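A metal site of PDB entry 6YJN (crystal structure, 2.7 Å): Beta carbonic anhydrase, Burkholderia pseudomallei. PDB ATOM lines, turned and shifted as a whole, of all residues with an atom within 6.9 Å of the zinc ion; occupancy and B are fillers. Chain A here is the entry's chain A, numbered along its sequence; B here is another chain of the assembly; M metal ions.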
ATOM      1  N   GLY A  45     -30.450   2.696 -23.565  1.00  0.00           N
ATOM      2  CA  GLY A  45     -30.514   4.102 -23.898  1.00  0.00           C
ATOM      3  C   GLY A  45     -29.728   4.975 -22.929  1.00  0.00           C
ATOM      4  O   GLY A  45     -28.948   4.487 -22.092  1.00  0.00           O
ATOM      5  N   CYS A  46     -29.961   6.280 -23.052  1.00  0.00           N
ATOM      6  CA  CYS A  46     -29.184   7.262 -22.314  1.00  0.00           C
ATOM      7  C   CYS A  46     -29.949   7.666 -21.053  1.00  0.00           C
ATOM      8  O   CYS A  46     -31.172   7.640 -21.028  1.00  0.00           O
ATOM      9  CB  CYS A  46     -28.890   8.459 -23.196  1.00  0.00           C
ATOM     10  SG  CYS A  46     -28.263   9.823 -22.207  1.00  0.00           S
ATOM     11  N   SER A  47     -29.198   8.038 -20.015  1.00  0.00           N
ATOM     12  CA  SER A  47     -29.807   8.409 -18.746  1.00  0.00           C
ATOM     13  C   SER A  47     -30.518   9.762 -18.867  1.00  0.00           C
ATOM     14  O   SER A  47     -31.324  10.077 -17.995  1.00  0.00           O
ATOM     15  CB  SER A  47     -28.834   8.387 -17.601  1.00  0.00           C
ATOM     16  OG  SER A  47     -28.480   7.049 -17.263  1.00  0.00           O
ATOM     17  N   ASP A  48     -30.208  10.532 -19.914  1.00  0.00           N
ATOM     18  CA  ASP A  48     -31.085  11.595 -20.392  1.00  0.00           C
ATOM     19  C   ASP A  48     -32.372  10.942 -20.845  1.00  0.00           C
ATOM     20  O   ASP A  48     -32.597  10.749 -22.045  1.00  0.00           O
ATOM     21  CB  ASP A  48     -30.574  12.295 -21.646  1.00  0.00           C
ATOM     22  CG  ASP A  48     -29.238  12.968 -21.476  1.00  0.00           C
ATOM     23  OD1 ASP A  48     -28.998  13.439 -20.375  1.00  0.00           O
ATOM     24  OD2 ASP A  48     -28.427  12.969 -22.438  1.00  0.00           O
ATOM     25  N   SER A  49     -33.199  10.575 -19.878  1.00  0.00           N
ATOM     26  CA  SER A  49     -34.425   9.864 -20.176  1.00  0.00           C
ATOM     27  C   SER A  49     -35.450  10.901 -20.622  1.00  0.00           C
ATOM     28  O   SER A  49     -36.411  11.194 -19.904  1.00  0.00           O
ATOM     29  CB  SER A  49     -34.849   9.035 -18.998  1.00  0.00           C
ATOM     30  OG  SER A  49     -33.706   8.462 -18.387  1.00  0.00           O
ATOM     31  N   ASN A  69     -27.523   4.138 -19.186  1.00  0.00           N
ATOM     32  CA  ASN A  69     -26.281   4.717 -18.692  1.00  0.00           C
ATOM     33  C   ASN A  69     -26.014   6.017 -19.442  1.00  0.00           C
ATOM     34  O   ASN A  69     -26.637   6.291 -20.466  1.00  0.00           O
ATOM     35  CB  ASN A  69     -25.120   3.734 -18.830  1.00  0.00           C
ATOM     36  CG  ASN A  69     -24.775   3.432 -20.272  1.00  0.00           C
ATOM     37  OD1 ASN A  69     -24.261   4.294 -20.986  1.00  0.00           O
ATOM     38  ND2 ASN A  69     -25.012   2.195 -20.694  1.00  0.00           N
ATOM     39  N   ILE A  70     -25.058   6.822 -18.940  1.00  0.00           N
ATOM     40  CA  ILE A  70     -24.778   8.101 -19.572  1.00  0.00           C
ATOM     41  C   ILE A  70     -24.172   7.858 -20.956  1.00  0.00           C
ATOM     42  O   ILE A  70     -23.069   7.329 -21.065  1.00  0.00           O
ATOM     43  CB  ILE A  70     -24.052   9.152 -18.678  1.00  0.00           C
ATOM     44  CG1 ILE A  70     -22.875   9.849 -19.392  1.00  0.00           C
ATOM     45  CG2 ILE A  70     -23.673   8.640 -17.290  1.00  0.00           C
ATOM     46  N   ALA A  71     -24.982   8.144 -21.982  1.00  0.00           N
ATOM     47  CA  ALA A  71     -24.649   8.129 -23.397  1.00  0.00           C
ATOM     48  C   ALA A  71     -24.823   6.746 -23.995  1.00  0.00           C
ATOM     49  O   ALA A  71     -24.267   6.453 -25.050  1.00  0.00           O
ATOM     50  CB  ALA A  71     -23.260   8.659 -23.635  1.00  0.00           C
ATOM     51  N   ASN A  72     -25.624   5.887 -23.328  1.00  0.00           N
ATOM     52  CA  ASN A  72     -25.932   4.581 -23.870  1.00  0.00           C
ATOM     53  C   ASN A  72     -24.652   3.926 -24.407  1.00  0.00           C
ATOM     54  O   ASN A  72     -24.546   3.620 -25.589  1.00  0.00           O
ATOM     55  CB  ASN A  72     -27.026   4.640 -24.945  1.00  0.00           C
ATOM     56  CG  ASN A  72     -26.755   5.671 -26.025  1.00  0.00           C
ATOM     57  OD1 ASN A  72     -27.328   6.755 -25.996  1.00  0.00           O
ATOM     58  ND2 ASN A  72     -25.882   5.339 -26.979  1.00  0.00           N
ATOM     59  N   GLY A 101     -29.641   5.918 -29.212  1.00  0.00           N
ATOM     60  CA  GLY A 101     -29.155   7.245 -28.891  1.00  0.00           C
ATOM     61  C   GLY A 101     -30.241   8.312 -29.108  1.00  0.00           C
ATOM     62  O   GLY A 101     -31.322   8.010 -29.599  1.00  0.00           O
ATOM     63  N   HIS A 102     -29.938   9.553 -28.718  1.00  0.00           N
ATOM     64  CA  HIS A 102     -30.941  10.602 -28.684  1.00  0.00           C
ATOM     65  C   HIS A 102     -30.317  11.973 -28.950  1.00  0.00           C
ATOM     66  O   HIS A 102     -29.376  12.399 -28.270  1.00  0.00           O
ATOM     67  CB  HIS A 102     -31.710  10.474 -27.364  1.00  0.00           C
ATOM     68  CG  HIS A 102     -31.062  11.178 -26.227  1.00  0.00           C
ATOM     69  ND1 HIS A 102     -31.317  12.495 -25.928  1.00  0.00           N
ATOM     70  CD2 HIS A 102     -30.143  10.760 -25.336  1.00  0.00           C
ATOM     71  CE1 HIS A 102     -30.594  12.862 -24.900  1.00  0.00           C
ATOM     72  NE2 HIS A 102     -29.869  11.807 -24.512  1.00  0.00           N
ATOM     73  N   TYR A 103     -30.862  12.687 -29.949  1.00  0.00           N
ATOM     74  CA  TYR A 103     -30.300  13.958 -30.373  1.00  0.00           C
ATOM     75  C   TYR A 103     -30.290  14.948 -29.224  1.00  0.00           C
ATOM     76  O   TYR A 103     -31.276  15.038 -28.477  1.00  0.00           O
ATOM     77  CB  TYR A 103     -31.018  14.543 -31.597  1.00  0.00           C
ATOM     78  CG  TYR A 103     -30.790  13.744 -32.842  1.00  0.00           C
ATOM     79  CD1 TYR A 103     -29.532  13.639 -33.409  1.00  0.00           C
ATOM     80  CD2 TYR A 103     -31.837  13.052 -33.449  1.00  0.00           C
ATOM     81  CE1 TYR A 103     -29.306  12.882 -34.555  1.00  0.00           C
ATOM     82  CE2 TYR A 103     -31.632  12.301 -34.600  1.00  0.00           C
ATOM     83  CZ  TYR A 103     -30.364  12.215 -35.146  1.00  0.00           C
ATOM     84  OH  TYR A 103     -30.170  11.490 -36.282  1.00  0.00           O
ATOM     85  N   GLY A 104     -29.165  15.655 -29.090  1.00  0.00           N
ATOM     86  CA  GLY A 104     -28.991  16.665 -28.068  1.00  0.00           C
ATOM     87  C   GLY A 104     -28.693  16.060 -26.701  1.00  0.00           C
ATOM     88  O   GLY A 104     -28.944  16.712 -25.693  1.00  0.00           O
ATOM     89  N   CYS A 105     -28.183  14.817 -26.711  1.00  0.00           N
ATOM     90  CA  CYS A 105     -27.708  14.093 -25.551  1.00  0.00           C
ATOM     91  C   CYS A 105     -26.580  14.862 -24.852  1.00  0.00           C
ATOM     92  O   CYS A 105     -25.587  15.215 -25.476  1.00  0.00           O
ATOM     93  CB  CYS A 105     -27.153  12.722 -25.956  1.00  0.00           C
ATOM     94  SG  CYS A 105     -26.610  11.720 -24.541  1.00  0.00           S
ATOM     95  N   SER A 106     -26.748  15.060 -23.537  1.00  0.00           N
ATOM     96  CA  SER A 106     -25.862  15.863 -22.709  1.00  0.00           C
ATOM     97  C   SER A 106     -24.490  15.209 -22.573  1.00  0.00           C
ATOM     98  O   SER A 106     -23.483  15.904 -22.436  1.00  0.00           O
ATOM     99  CB  SER A 106     -26.487  16.002 -21.362  1.00  0.00           C
ATOM    100  OG  SER A 106     -26.436  14.762 -20.678  1.00  0.00           O
ATOM    101  N   GLY A 107     -24.483  13.867 -22.522  1.00  0.00           N
ATOM    102  CA  GLY A 107     -23.276  13.065 -22.505  1.00  0.00           C
ATOM    103  C   GLY A 107     -22.439  13.284 -23.764  1.00  0.00           C
ATOM    104  O   GLY A 107     -21.293  13.687 -23.670  1.00  0.00           O
ATOM    105  N   VAL A 108     -23.055  13.041 -24.940  1.00  0.00           N
ATOM    106  CA  VAL A 108     -22.365  13.119 -26.224  1.00  0.00           C
ATOM    107  C   VAL A 108     -21.869  14.539 -26.439  1.00  0.00           C
ATOM    108  O   VAL A 108     -20.858  14.738 -27.114  1.00  0.00           O
ATOM    109  CB  VAL A 108     -23.246  12.664 -27.394  1.00  0.00           C
ATOM    110  CG1 VAL A 108     -22.517  12.846 -28.722  1.00  0.00           C
ATOM    111  CG2 VAL A 108     -23.714  11.222 -27.242  1.00  0.00           C
ATOM    112  N   PHE B  65     -33.997  11.957 -14.167  1.00  0.00           N
ATOM    113  CA  PHE B  65     -32.793  11.354 -14.703  1.00  0.00           C
ATOM    114  C   PHE B  65     -32.716   9.902 -14.236  1.00  0.00           C
ATOM    115  O   PHE B  65     -32.872   9.622 -13.049  1.00  0.00           O
ATOM    116  CB  PHE B  65     -31.587  12.154 -14.198  1.00  0.00           C
ATOM    117  CG  PHE B  65     -30.355  12.094 -15.065  1.00  0.00           C
ATOM    118  CD1 PHE B  65     -30.390  12.510 -16.393  1.00  0.00           C
ATOM    119  CD2 PHE B  65     -29.157  11.639 -14.544  1.00  0.00           C
ATOM    120  CE1 PHE B  65     -29.258  12.450 -17.194  1.00  0.00           C
ATOM    121  CE2 PHE B  65     -28.026  11.580 -15.345  1.00  0.00           C
ATOM    122  CZ  PHE B  65     -28.076  11.988 -16.658  1.00  0.00           C
HETATM  123 ZN    ZN M   1     -28.370  11.394 -23.488  1.00  0.00          ZN
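The side-chain sulfur (SG) of Cys 46 sits close to the backbone NH (N) of Ala 71 (3.7 Å). The side-chain sulfur (SG) of Cys 105 lies close to the backbone NH (N) of Gly 107 (3.6 Å). OG of Ser 106 lies within hydrogen-bond range of OD1 of Asp 48, 2.9 Å away.
Within 4 Å of the zinc ion: Cys 46, Asp 48, His 102 and Cys 105. The nearest printed residue that does not touch the zinc ion is Ser 106 (4.01 Å).
The zinc ion is bound by NE2 of His 102 (1.9 Å). The side-chain carboxylate (OD2) of Asp 48 is bound to the zinc ion, at 1.9 Å. SG of Cys 46 binds the zinc ion (2.0 Å). SG of Cys 105 binds the zinc ion, 2.1 Å away. The zinc ion has four donor atoms within binding distance.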
